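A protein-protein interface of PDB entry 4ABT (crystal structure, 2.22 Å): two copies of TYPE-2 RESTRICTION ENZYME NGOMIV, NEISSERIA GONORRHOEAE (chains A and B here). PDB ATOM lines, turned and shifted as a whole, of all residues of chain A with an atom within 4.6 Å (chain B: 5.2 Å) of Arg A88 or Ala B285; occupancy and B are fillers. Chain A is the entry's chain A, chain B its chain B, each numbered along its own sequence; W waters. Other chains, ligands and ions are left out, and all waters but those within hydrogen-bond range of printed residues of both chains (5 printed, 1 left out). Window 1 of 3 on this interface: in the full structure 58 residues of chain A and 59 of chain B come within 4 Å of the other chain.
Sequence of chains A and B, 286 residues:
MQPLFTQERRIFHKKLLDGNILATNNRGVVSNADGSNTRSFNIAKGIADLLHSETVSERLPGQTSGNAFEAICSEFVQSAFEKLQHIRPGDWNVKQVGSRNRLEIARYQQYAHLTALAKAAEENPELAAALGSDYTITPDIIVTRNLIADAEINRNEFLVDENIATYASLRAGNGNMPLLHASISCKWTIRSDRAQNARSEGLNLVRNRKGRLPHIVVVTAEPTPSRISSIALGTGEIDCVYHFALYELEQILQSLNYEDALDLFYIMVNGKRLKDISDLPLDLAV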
ATOM      1  N   PHE A  81      38.351 -31.393  -7.002  1.00  0.00           N
ATOM      2  CA  PHE A  81      37.180 -30.479  -6.991  1.00  0.00           C
ATOM      3  C   PHE A  81      37.532 -28.998  -7.006  1.00  0.00           C
ATOM      4  O   PHE A  81      36.800 -28.197  -7.588  1.00  0.00           O
ATOM      5  CB  PHE A  81      36.323 -30.706  -5.755  1.00  0.00           C
ATOM      6  CG  PHE A  81      34.977 -30.054  -5.817  1.00  0.00           C
ATOM      7  CD1 PHE A  81      34.042 -30.450  -6.782  1.00  0.00           C
ATOM      8  CD2 PHE A  81      34.633 -29.054  -4.909  1.00  0.00           C
ATOM      9  CE1 PHE A  81      32.793 -29.866  -6.837  1.00  0.00           C
ATOM     10  CE2 PHE A  81      33.354 -28.450  -4.944  1.00  0.00           C
ATOM     11  CZ  PHE A  81      32.431 -28.864  -5.899  1.00  0.00           C
ATOM     12  N   LEU A  84      37.531 -27.044 -10.345  1.00  0.00           N
ATOM     13  CA  LEU A  84      36.212 -26.934 -11.029  1.00  0.00           C
ATOM     14  C   LEU A  84      35.405 -25.663 -10.657  1.00  0.00           C
ATOM     15  O   LEU A  84      34.165 -25.628 -10.766  1.00  0.00           O
ATOM     16  CB  LEU A  84      35.405 -28.216 -10.788  1.00  0.00           C
ATOM     17  CG  LEU A  84      36.004 -29.524 -11.342  1.00  0.00           C
ATOM     18  CD1 LEU A  84      35.110 -30.769 -11.055  1.00  0.00           C
ATOM     19  CD2 LEU A  84      36.233 -29.358 -12.816  1.00  0.00           C
ATOM     20  N   GLN A  85      36.113 -24.598 -10.271  1.00  0.00           N
ATOM     21  CA  GLN A  85      35.500 -23.409  -9.711  1.00  0.00           C
ATOM     22  C   GLN A  85      34.711 -22.663 -10.774  1.00  0.00           C
ATOM     23  O   GLN A  85      33.751 -21.963 -10.467  1.00  0.00           O
ATOM     24  CB  GLN A  85      36.588 -22.479  -9.162  1.00  0.00           C
ATOM     25  CG  GLN A  85      37.064 -22.804  -7.783  1.00  0.00           C
ATOM     26  CD  GLN A  85      36.100 -22.331  -6.698  1.00  0.00           C
ATOM     27  OE1 GLN A  85      36.055 -22.923  -5.610  1.00  0.00           O
ATOM     28  NE2 GLN A  85      35.338 -21.251  -6.979  1.00  0.00           N
ATOM     29  N   HIS A  86      35.130 -22.823 -12.021  1.00  0.00           N
ATOM     30  CA  HIS A  86      34.511 -22.190 -13.151  1.00  0.00           C
ATOM     31  C   HIS A  86      33.239 -22.926 -13.566  1.00  0.00           C
ATOM     32  O   HIS A  86      32.344 -22.335 -14.190  1.00  0.00           O
ATOM     33  CB  HIS A  86      35.520 -22.134 -14.299  1.00  0.00           C
ATOM     34  CG  HIS A  86      36.090 -23.480 -14.660  1.00  0.00           C
ATOM     35  ND1 HIS A  86      35.831 -24.097 -15.860  1.00  0.00           N
ATOM     36  CD2 HIS A  86      36.876 -24.331 -13.966  1.00  0.00           C
ATOM     37  CE1 HIS A  86      36.456 -25.257 -15.899  1.00  0.00           C
ATOM     38  NE2 HIS A  86      37.089 -25.421 -14.760  1.00  0.00           N
ATOM     39  N   ILE A  87      33.108 -24.191 -13.212  1.00  0.00           N
ATOM     40  CA  ILE A  87      31.795 -24.836 -13.462  1.00  0.00           C
ATOM     41  C   ILE A  87      30.902 -25.031 -12.228  1.00  0.00           C
ATOM     42  O   ILE A  87      29.709 -25.233 -12.381  1.00  0.00           O
ATOM     43  CB  ILE A  87      31.914 -26.197 -14.194  1.00  0.00           C
ATOM     44  CG1 ILE A  87      32.720 -27.174 -13.392  1.00  0.00           C
ATOM     45  CG2 ILE A  87      32.530 -26.042 -15.639  1.00  0.00           C
ATOM     46  CD1 ILE A  87      32.639 -28.575 -13.984  1.00  0.00           C
ATOM     47  N   ARG A  88      31.487 -25.002 -11.024  1.00  0.00           N
ATOM     48  CA  ARG A  88      30.771 -25.064  -9.762  1.00  0.00           C
ATOM     49  C   ARG A  88      31.439 -24.154  -8.710  1.00  0.00           C
ATOM     50  O   ARG A  88      32.102 -24.625  -7.782  1.00  0.00           O
ATOM     51  CB  ARG A  88      30.709 -26.493  -9.251  1.00  0.00           C
ATOM     52  CG  ARG A  88      29.576 -26.691  -8.184  1.00  0.00           C
ATOM     53  CD  ARG A  88      28.166 -26.488  -8.840  1.00  0.00           C
ATOM     54  NE  ARG A  88      27.131 -27.141  -8.025  1.00  0.00           N
ATOM     55  CZ  ARG A  88      26.455 -26.531  -7.052  1.00  0.00           C
ATOM     56  NH1 ARG A  88      26.687 -25.214  -6.776  1.00  0.00           N
ATOM     57  NH2 ARG A  88      25.550 -27.235  -6.352  1.00  0.00           N
ATOM     58  N   PRO A  89      31.282 -22.823  -8.858  1.00  0.00           N
ATOM     59  CA  PRO A  89      31.979 -21.947  -7.911  1.00  0.00           C
ATOM     60  C   PRO A  89      31.467 -21.990  -6.496  1.00  0.00           C
ATOM     61  O   PRO A  89      30.287 -22.376  -6.247  1.00  0.00           O
ATOM     62  CB  PRO A  89      31.768 -20.539  -8.471  1.00  0.00           C
ATOM     63  CG  PRO A  89      30.561 -20.666  -9.389  1.00  0.00           C
ATOM     64  CD  PRO A  89      30.571 -22.077  -9.906  1.00  0.00           C
ATOM     65  N   GLY A  90      32.361 -21.572  -5.593  1.00  0.00           N
ATOM     66  CA  GLY A  90      32.029 -21.352  -4.208  1.00  0.00           C
ATOM     67  C   GLY A  90      33.185 -21.490  -3.234  1.00  0.00           C
ATOM     68  O   GLY A  90      34.342 -21.727  -3.616  1.00  0.00           O
ATOM     69  N   TRP A  92      34.409 -23.821  -0.664  1.00  0.00           N
ATOM     70  CA  TRP A  92      34.059 -25.213  -0.451  1.00  0.00           C
ATOM     71  C   TRP A  92      34.940 -25.703   0.606  1.00  0.00           C
ATOM     72  O   TRP A  92      36.076 -25.301   0.652  1.00  0.00           O
ATOM     73  CB  TRP A  92      34.282 -26.074  -1.731  1.00  0.00           C
ATOM     74  CG  TRP A  92      33.438 -25.670  -2.899  1.00  0.00           C
ATOM     75  CD1 TRP A  92      33.841 -24.966  -4.022  1.00  0.00           C
ATOM     76  CD2 TRP A  92      32.033 -25.945  -3.086  1.00  0.00           C
ATOM     77  NE1 TRP A  92      32.754 -24.782  -4.878  1.00  0.00           N
ATOM     78  CE2 TRP A  92      31.650 -25.378  -4.324  1.00  0.00           C
ATOM     79  CE3 TRP A  92      31.058 -26.608  -2.316  1.00  0.00           C
ATOM     80  CZ2 TRP A  92      30.363 -25.450  -4.789  1.00  0.00           C
ATOM     81  CZ3 TRP A  92      29.770 -26.699  -2.808  1.00  0.00           C
ATOM     82  CH2 TRP A  92      29.451 -26.150  -4.037  1.00  0.00           C
ATOM     83  N   ARG A 145      29.437 -26.097   1.660  1.00  0.00           N
ATOM     84  CA  ARG A 145      29.582 -24.810   1.007  1.00  0.00           C
ATOM     85  C   ARG A 145      29.355 -23.675   2.040  1.00  0.00           C
ATOM     86  O   ARG A 145      28.313 -23.654   2.708  1.00  0.00           O
ATOM     87  CB  ARG A 145      28.527 -24.679  -0.100  1.00  0.00           C
ATOM     88  CG  ARG A 145      28.831 -23.588  -1.052  1.00  0.00           C
ATOM     89  CD  ARG A 145      27.766 -23.433  -2.141  1.00  0.00           C
ATOM     90  NE  ARG A 145      28.042 -22.214  -2.910  1.00  0.00           N
ATOM     91  CZ  ARG A 145      27.530 -21.937  -4.094  1.00  0.00           C
ATOM     92  NH1 ARG A 145      26.663 -22.757  -4.669  1.00  0.00           N
ATOM     93  NH2 ARG A 145      27.871 -20.811  -4.693  1.00  0.00           N
ATOM     94  N   LEU A 170      21.607 -19.489   0.481  1.00  0.00           N
ATOM     95  CA  LEU A 170      22.999 -19.172   0.217  1.00  0.00           C
ATOM     96  C   LEU A 170      23.428 -17.843   0.808  1.00  0.00           C
ATOM     97  O   LEU A 170      24.618 -17.549   0.884  1.00  0.00           O
ATOM     98  CB  LEU A 170      23.222 -19.078  -1.285  1.00  0.00           C
ATOM     99  CG  LEU A 170      23.583 -20.357  -1.984  1.00  0.00           C
ATOM    100  CD1 LEU A 170      23.386 -20.161  -3.473  1.00  0.00           C
ATOM    101  CD2 LEU A 170      25.024 -20.685  -1.645  1.00  0.00           C
ATOM    102  N   HIS A 181      27.003 -29.963   0.934  1.00  0.00           N
ATOM    103  CA  HIS A 181      26.988 -30.232  -0.500  1.00  0.00           C
ATOM    104  C   HIS A 181      27.038 -31.751  -0.838  1.00  0.00           C
ATOM    105  O   HIS A 181      26.404 -32.200  -1.765  1.00  0.00           O
ATOM    106  CB  HIS A 181      28.203 -29.555  -1.147  1.00  0.00           C
ATOM    107  CG  HIS A 181      28.287 -29.749  -2.634  1.00  0.00           C
ATOM    108  ND1 HIS A 181      27.449 -29.101  -3.518  1.00  0.00           N
ATOM    109  CD2 HIS A 181      29.129 -30.483  -3.388  1.00  0.00           C
ATOM    110  CE1 HIS A 181      27.768 -29.436  -4.756  1.00  0.00           C
ATOM    111  NE2 HIS A 181      28.782 -30.280  -4.707  1.00  0.00           N
ATOM    112  N   LEU A 284      30.413 -34.077  -8.568  1.00  0.00           N
ATOM    113  CA  LEU A 284      30.083 -33.160  -7.474  1.00  0.00           C
ATOM    114  C   LEU A 284      29.867 -31.701  -7.938  1.00  0.00           C
ATOM    115  O   LEU A 284      29.524 -30.814  -7.112  1.00  0.00           O
ATOM    116  CB  LEU A 284      31.177 -33.205  -6.375  1.00  0.00           C
ATOM    117  CG  LEU A 284      31.390 -34.496  -5.575  1.00  0.00           C
ATOM    118  CD1 LEU A 284      32.648 -34.523  -4.775  1.00  0.00           C
ATOM    119  CD2 LEU A 284      30.220 -34.747  -4.652  1.00  0.00           C
ATOM    120  N   ALA A 285      30.087 -31.454  -9.233  1.00  0.00           N
ATOM    121  CA  ALA A 285      29.900 -30.145  -9.846  1.00  0.00           C
ATOM    122  C   ALA A 285      28.585 -30.027 -10.580  1.00  0.00           C
ATOM    123  O   ALA A 285      28.333 -29.011 -11.196  1.00  0.00           O
ATOM    124  CB  ALA A 285      31.016 -29.839 -10.816  1.00  0.00           C
ATOM    125  N   VAL A 286      27.738 -31.034 -10.496  1.00  0.00           N
ATOM    126  CA  VAL A 286      26.471 -30.994 -11.196  1.00  0.00           C
ATOM    127  C   VAL A 286      25.614 -29.817 -10.716  1.00  0.00           C
ATOM    128  O   VAL A 286      24.957 -29.141 -11.559  1.00  0.00           O
ATOM    129  CB  VAL A 286      25.742 -32.362 -11.072  1.00  0.00           C
ATOM    130  CG1 VAL A 286      24.258 -32.203 -11.367  1.00  0.00           C
ATOM    131  CG2 VAL A 286      26.396 -33.439 -12.012  1.00  0.00           C
ATOM    132  OXT VAL A 286      25.606 -29.502  -9.491  1.00  0.00           O
ATOM    133  N   PHE B  81      16.707 -16.508 -12.370  1.00  0.00           N
ATOM    134  CA  PHE B  81      17.822 -17.459 -12.338  1.00  0.00           C
ATOM    135  C   PHE B  81      19.025 -17.145 -13.279  1.00  0.00           C
ATOM    136  O   PHE B  81      20.162 -17.475 -12.978  1.00  0.00           O
ATOM    137  CB  PHE B  81      17.338 -18.911 -12.544  1.00  0.00           C
ATOM    138  CG  PHE B  81      18.382 -19.952 -12.244  1.00  0.00           C
ATOM    139  CD1 PHE B  81      18.937 -20.041 -10.998  1.00  0.00           C
ATOM    140  CD2 PHE B  81      18.816 -20.812 -13.224  1.00  0.00           C
ATOM    141  CE1 PHE B  81      19.916 -20.995 -10.696  1.00  0.00           C
ATOM    142  CE2 PHE B  81      19.786 -21.799 -12.948  1.00  0.00           C
ATOM    143  CZ  PHE B  81      20.334 -21.902 -11.676  1.00  0.00           C
ATOM    144  N   LEU B  84      22.004 -15.323 -11.979  1.00  0.00           N
ATOM    145  CA  LEU B  84      22.872 -15.989 -11.017  1.00  0.00           C
ATOM    146  C   LEU B  84      24.022 -16.785 -11.656  1.00  0.00           C
ATOM    147  O   LEU B  84      24.606 -17.667 -11.035  1.00  0.00           O
ATOM    148  CB  LEU B  84      22.046 -16.839 -10.047  1.00  0.00           C
ATOM    149  CG  LEU B  84      21.077 -15.888  -9.327  1.00  0.00           C
ATOM    150  CD1 LEU B  84      19.929 -16.678  -8.660  1.00  0.00           C
ATOM    151  CD2 LEU B  84      21.828 -15.007  -8.319  1.00  0.00           C
ATOM    152  N   ILE B  87      27.253 -17.409  -9.667  1.00  0.00           N
ATOM    153  CA  ILE B  87      27.129 -18.235  -8.452  1.00  0.00           C
ATOM    154  C   ILE B  87      26.819 -19.692  -8.818  1.00  0.00           C
ATOM    155  O   ILE B  87      27.107 -20.628  -8.029  1.00  0.00           O
ATOM    156  CB  ILE B  87      25.956 -17.721  -7.593  1.00  0.00           C
ATOM    157  CG1 ILE B  87      26.267 -16.330  -7.095  1.00  0.00           C
ATOM    158  CG2 ILE B  87      25.753 -18.542  -6.370  1.00  0.00           C
ATOM    159  CD1 ILE B  87      27.545 -16.299  -6.368  1.00  0.00           C
ATOM    160  N   ARG B  88      26.193 -19.850 -10.005  1.00  0.00           N
ATOM    161  CA  ARG B  88      25.705 -21.136 -10.519  1.00  0.00           C
ATOM    162  C   ARG B  88      25.752 -21.125 -12.043  1.00  0.00           C
ATOM    163  O   ARG B  88      24.725 -20.977 -12.699  1.00  0.00           O
ATOM    164  CB  ARG B  88      24.292 -21.492  -9.995  1.00  0.00           C
ATOM    165  CG  ARG B  88      23.946 -22.964 -10.074  1.00  0.00           C
ATOM    166  CD  ARG B  88      24.902 -23.820  -9.205  1.00  0.00           C
ATOM    167  NE  ARG B  88      24.289 -25.101  -8.821  1.00  0.00           N
ATOM    168  CZ  ARG B  88      24.438 -26.215  -9.538  1.00  0.00           C
ATOM    169  NH1 ARG B  88      25.220 -26.196 -10.630  1.00  0.00           N
ATOM    170  NH2 ARG B  88      23.841 -27.338  -9.143  1.00  0.00           N
ATOM    171  N   PRO B  89      26.958 -21.243 -12.619  1.00  0.00           N
ATOM    172  CA  PRO B  89      27.012 -21.202 -14.093  1.00  0.00           C
ATOM    173  C   PRO B  89      26.546 -22.524 -14.751  1.00  0.00           C
ATOM    174  O   PRO B  89      26.424 -23.576 -14.074  1.00  0.00           O
ATOM    175  CB  PRO B  89      28.488 -20.883 -14.404  1.00  0.00           C
ATOM    176  CG  PRO B  89      29.201 -21.360 -13.212  1.00  0.00           C
ATOM    177  CD  PRO B  89      28.289 -21.135 -12.015  1.00  0.00           C
ATOM    178  N   ARG B 145      20.076 -28.599 -17.228  1.00  0.00           N
ATOM    179  CA  ARG B 145      21.429 -28.149 -17.531  1.00  0.00           C
ATOM    180  C   ARG B 145      21.957 -29.095 -18.611  1.00  0.00           C
ATOM    181  O   ARG B 145      22.001 -30.282 -18.394  1.00  0.00           O
ATOM    182  CB  ARG B 145      22.297 -28.293 -16.265  1.00  0.00           C
ATOM    183  CG  ARG B 145      23.631 -27.704 -16.408  1.00  0.00           C
ATOM    184  CD  ARG B 145      24.480 -28.042 -15.318  1.00  0.00           C
ATOM    185  NE  ARG B 145      25.732 -27.379 -15.563  1.00  0.00           N
ATOM    186  CZ  ARG B 145      26.698 -27.265 -14.666  1.00  0.00           C
ATOM    187  NH1 ARG B 145      26.530 -27.788 -13.452  1.00  0.00           N
ATOM    188  NH2 ARG B 145      27.831 -26.621 -14.965  1.00  0.00           N
ATOM    189  N   HIS B 181      17.796 -30.331 -13.301  1.00  0.00           N
ATOM    190  CA  HIS B 181      18.252 -29.515 -12.198  1.00  0.00           C
ATOM    191  C   HIS B 181      17.122 -29.299 -11.173  1.00  0.00           C
ATOM    192  O   HIS B 181      17.371 -29.360  -9.992  1.00  0.00           O
ATOM    193  CB  HIS B 181      18.722 -28.146 -12.743  1.00  0.00           C
ATOM    194  CG  HIS B 181      19.184 -27.182 -11.690  1.00  0.00           C
ATOM    195  ND1 HIS B 181      20.269 -27.431 -10.885  1.00  0.00           N
ATOM    196  CD2 HIS B 181      18.741 -25.940 -11.353  1.00  0.00           C
ATOM    197  CE1 HIS B 181      20.468 -26.402 -10.076  1.00  0.00           C
ATOM    198  NE2 HIS B 181      19.559 -25.479 -10.344  1.00  0.00           N
ATOM    199  N   ARG B 212      22.462 -37.234  -8.794  1.00  0.00           N
ATOM    200  CA  ARG B 212      22.048 -36.250  -7.803  1.00  0.00           C
ATOM    201  C   ARG B 212      20.581 -35.915  -7.981  1.00  0.00           C
ATOM    202  O   ARG B 212      20.117 -35.683  -9.118  1.00  0.00           O
ATOM    203  CB  ARG B 212      22.869 -34.942  -7.875  1.00  0.00           C
ATOM    204  CG  ARG B 212      22.683 -34.136  -6.553  1.00  0.00           C
ATOM    205  CD  ARG B 212      22.908 -32.633  -6.572  1.00  0.00           C
ATOM    206  NE  ARG B 212      22.805 -32.069  -5.201  1.00  0.00           N
ATOM    207  CZ  ARG B 212      23.313 -30.875  -4.801  1.00  0.00           C
ATOM    208  NH1 ARG B 212      23.976 -30.087  -5.659  1.00  0.00           N
ATOM    209  NH2 ARG B 212      23.158 -30.443  -3.536  1.00  0.00           N
ATOM    210  N   HIS B 215      16.467 -30.307  -7.364  1.00  0.00           N
ATOM    211  CA  HIS B 215      15.628 -29.502  -6.490  1.00  0.00           C
ATOM    212  C   HIS B 215      14.191 -29.955  -6.632  1.00  0.00           C
ATOM    213  O   HIS B 215      13.760 -30.200  -7.703  1.00  0.00           O
ATOM    214  CB  HIS B 215      15.717 -28.007  -6.847  1.00  0.00           C
ATOM    215  CG  HIS B 215      17.064 -27.395  -6.574  1.00  0.00           C
ATOM    216  ND1 HIS B 215      18.100 -27.407  -7.497  1.00  0.00           N
ATOM    217  CD2 HIS B 215      17.545 -26.758  -5.491  1.00  0.00           C
ATOM    218  CE1 HIS B 215      19.152 -26.786  -6.997  1.00  0.00           C
ATOM    219  NE2 HIS B 215      18.851 -26.407  -5.768  1.00  0.00           N
ATOM    220  N   PRO B 281      14.922 -18.345  -6.969  1.00  0.00           N
ATOM    221  CA  PRO B 281      16.054 -18.323  -7.870  1.00  0.00           C
ATOM    222  C   PRO B 281      17.356 -18.594  -7.187  1.00  0.00           C
ATOM    223  O   PRO B 281      18.157 -19.381  -7.687  1.00  0.00           O
ATOM    224  CB  PRO B 281      16.036 -16.881  -8.380  1.00  0.00           C
ATOM    225  CG  PRO B 281      14.646 -16.520  -8.368  1.00  0.00           C
ATOM    226  CD  PRO B 281      14.106 -17.127  -7.120  1.00  0.00           C
ATOM    227  N   LEU B 282      17.584 -17.957  -6.048  1.00  0.00           N
ATOM    228  CA  LEU B 282      18.786 -18.175  -5.283  1.00  0.00           C
ATOM    229  C   LEU B 282      18.844 -19.573  -4.697  1.00  0.00           C
ATOM    230  O   LEU B 282      19.957 -20.127  -4.596  1.00  0.00           O
ATOM    231  CB  LEU B 282      18.990 -17.125  -4.179  1.00  0.00           C
ATOM    232  CG  LEU B 282      19.857 -15.952  -4.647  1.00  0.00           C
ATOM    233  CD1 LEU B 282      19.593 -14.738  -3.793  1.00  0.00           C
ATOM    234  CD2 LEU B 282      21.343 -16.303  -4.604  1.00  0.00           C
ATOM    235  N   ASP B 283      17.692 -20.148  -4.307  1.00  0.00           N
ATOM    236  CA  ASP B 283      17.719 -21.527  -3.794  1.00  0.00           C
ATOM    237  C   ASP B 283      18.070 -22.553  -4.888  1.00  0.00           C
ATOM    238  O   ASP B 283      18.532 -23.660  -4.580  1.00  0.00           O
ATOM    239  CB  ASP B 283      16.425 -21.868  -3.057  1.00  0.00           C
ATOM    240  CG  ASP B 283      16.421 -21.336  -1.588  1.00  0.00           C
ATOM    241  OD1 ASP B 283      17.449 -20.728  -1.193  1.00  0.00           O
ATOM    242  OD2 ASP B 283      15.383 -21.476  -0.854  1.00  0.00           O
ATOM    243  N   LEU B 284      17.871 -22.169  -6.156  1.00  0.00           N
ATOM    244  CA  LEU B 284      18.247 -22.982  -7.310  1.00  0.00           C
ATOM    245  C   LEU B 284      19.738 -22.907  -7.655  1.00  0.00           C
ATOM    246  O   LEU B 284      20.200 -23.622  -8.541  1.00  0.00           O
ATOM    247  CB  LEU B 284      17.405 -22.611  -8.560  1.00  0.00           C
ATOM    248  CG  LEU B 284      15.939 -22.989  -8.369  1.00  0.00           C
ATOM    249  CD1 LEU B 284      15.082 -22.437  -9.487  1.00  0.00           C
ATOM    250  CD2 LEU B 284      15.731 -24.565  -8.216  1.00  0.00           C
ATOM    251  N   ALA B 285      20.464 -22.017  -6.967  1.00  0.00           N
ATOM    252  CA  ALA B 285      21.904 -21.841  -7.148  1.00  0.00           C
ATOM    253  C   ALA B 285      22.766 -22.572  -6.120  1.00  0.00           C
ATOM    254  O   ALA B 285      23.991 -22.520  -6.195  1.00  0.00           O
ATOM    255  CB  ALA B 285      22.244 -20.354  -7.136  1.00  0.00           C
ATOM    256  N   VAL B 286      22.145 -23.219  -5.135  1.00  0.00           N
ATOM    257  CA  VAL B 286      22.894 -23.771  -3.999  1.00  0.00           C
ATOM    258  C   VAL B 286      23.991 -24.749  -4.472  1.00  0.00           C
ATOM    259  O   VAL B 286      25.117 -24.884  -3.957  1.00  0.00           O
ATOM    260  CB  VAL B 286      21.930 -24.471  -3.001  1.00  0.00           C
ATOM    261  CG1 VAL B 286      22.664 -25.523  -2.170  1.00  0.00           C
ATOM    262  CG2 VAL B 286      21.247 -23.475  -2.154  1.00  0.00           C
ATOM    263  OXT VAL B 286      23.745 -25.471  -5.436  1.00  0.00           O
HETATM  264  O   HOH W   1      22.115 -29.499 -11.816  1.00  0.00           O
HETATM  265  O   HOH W   2      25.474 -27.228  -2.902  1.00  0.00           O
HETATM  266  O   HOH W   3      19.979 -19.688  -1.831  1.00  0.00           O
HETATM  267  O   HOH W   4      28.188 -23.257  -7.819  1.00  0.00           O
HETATM  268  O   HOH W   5      27.117 -24.419 -11.655  1.00  0.00           O
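Arg A88 touches its own counterpart, Arg B88.
Arg A88 touches Ala B285, but with the chains exchanged Ala A285 does not touch Arg B88 (4.2 Å).
Arg A145 touches Ala B285, and with the chains exchanged Ala A285 touches Arg B145.
Arg A145 touches Val B286, and with the chains exchanged Val A286 touches Arg B145.
Of the 19 pairs that touch across the chains among the printed residues, 12 have their exchanged pair printed and touching as well.
The guanidinium group (NH2) of Arg B145 lies within hydrogen-bond range of the backbone carbonyl oxygen (O) of Ile A87 (3.5 Å).
The guanidinium group of Arg A88 is in salt-bridge range of the chain-end carboxylate of Val B286, at 2.7 Å.
NH2 of Arg A145 sits at hydrogen-bond distance from O of Ile B87, 3.4 Å away.
The backbone carbonyl oxygen (O) of Ala B285 lies within hydrogen-bond range of the guanidinium group (NH1) of Arg A145 (3.1 Å).
The guanidinium group of Arg A145 lies within salt-bridge range of the chain-end carboxylate of Val B286 (2.7 Å).
O of Ala A285 lies within hydrogen-bond range of NH1 of Arg B145 (3.1 Å).
The chain-end carboxylate (OXT) of Val A286 is in salt-bridge range of the guanidinium group (NH2) of Arg B88, at 2.8 Å.
O of Val A286 lies within salt-bridge range of NH1 of Arg B145, at 2.8 Å.
The guanidinium group of Arg A88 lies close to the guanidinium group of Arg B88.
The guanidinium group (NH1) of Arg B212 lies close to the guanidinium group (NH2) of Arg A88 (3.3 Å).
Hydrophobic or aromatic side chains of chain A that line the printed part of chain B: Pro A89, Leu A170 and His A181.
Hydrophobic or aromatic side chains of chain B that line the printed part of chain A: Ile B87, Pro B89, Ala B285 and Val B286.
Among the printed residues, no Asp or Glu carboxylate lies within 4 Å of a Lys or Arg side-chain nitrogen of the other chain.
O of His A86 touches CG of Pro B89, at 3.4 Å.
Ile A87 touches Pro B89 (O to CG, 3.99 Å).
O of Ala B285 touches NH1 of Arg A88 (3.9 Å).
O of Ile B87 touches CG of Pro A89, at 3.7 Å.
Pro A89 touches Pro B89 (CD to CD, 3.2 Å).
Leu A170 touches Leu B282 (CD1 to O, 3.6 Å).
Ala B285 touches Leu A170.
Leu A170 touches Val B286 (CD1 to CA, 3.7 Å).
Arg B212 touches His A181 (NH1 to CE1, 3.95 Å).
NE1 of Trp A92 lies within hydrogen-bond range of O of Arg A88 (3.0 Å).
The guanidinium group (NE) of Arg A88 lies within salt-bridge range of the chain-end carboxylate (OXT) of Val A286.
NH2 of Arg A145 lies within hydrogen-bond range of O of Pro A89 (3.3 Å).
A ring nitrogen (NE2) of His A181 is in hydrogen-bond range of the backbone carbonyl oxygen (O) of Leu A284.
The guanidinium group (NE) of Arg B88 lies within salt-bridge range of the chain-end carboxylate (OXT) of Val B286 (3.4 Å).
The backbone carbonyl oxygen (O) of Pro B89 lies within hydrogen-bond range of the guanidinium group (NH2) of Arg B145 (3.5 Å).
Water W2 lies within hydrogen-bond range of the chain-end carboxylate (O) of Val B286 (2.6 Å), a ring nitrogen (ND1) of His A181 (2.8 Å) and the guanidinium group (NH2) of Arg A88 (3.5 Å).
Water W5 lies within hydrogen-bond range of the backbone carbonyl oxygen (O) of Pro B89, the guanidinium group (NH1) of Arg B88 and the backbone carbonyl oxygen (O) of Ile A87.
Water W4 lies within hydrogen-bond range of NH1 of Arg A88 (2.7 Å), O of Pro A89 (2.8 Å) and O of Ile B87 (2.9 Å).
Water W3 lies within hydrogen-bond range of the backbone carbonyl oxygen of Leu B282, the side-chain carboxylate of Asp B283 and the backbone NH of Leu A170.
Water W1 lies within hydrogen-bond range of O of Val A286 (2.9 Å) and ND1 of His B181 (2.9 Å).
Printed residues of chain B within 4 Å of Arg A88: Arg B88 (3.1 Å), Arg B212 (3.3 Å), Ala B285 (3.9 Å) and Val B286 (2.7 Å).
Of chain A, only Arg A88, Arg A145 and Leu A170 come within 4 Å of Ala B285.
Of the printed residues of chain B, Val A286 touches Arg B88 (2.8 Å) and Arg B145 (2.8 Å).
Of the printed residues of chain B, Leu A170 touches Leu B282, Ala B285 and Val B286.
Printed residues of chain B within 4 Å of Pro A89: Ile B87 (3.7 Å) and Pro B89 (3.2 Å).
Printed residues of chain A within 4 Å of Val B286: Arg A88, Arg A145 and Leu A170.
Printed residues of chain A within 4 Å of Arg B88: Arg A88 and Val A286.
Leu A84 touches none of the printed residues of chain B.
Pro B281 touches none of the printed residues of chain A.
The nearest printed residue of chain A that does not touch Ala B285 is Pro A89 (6.3 Å).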
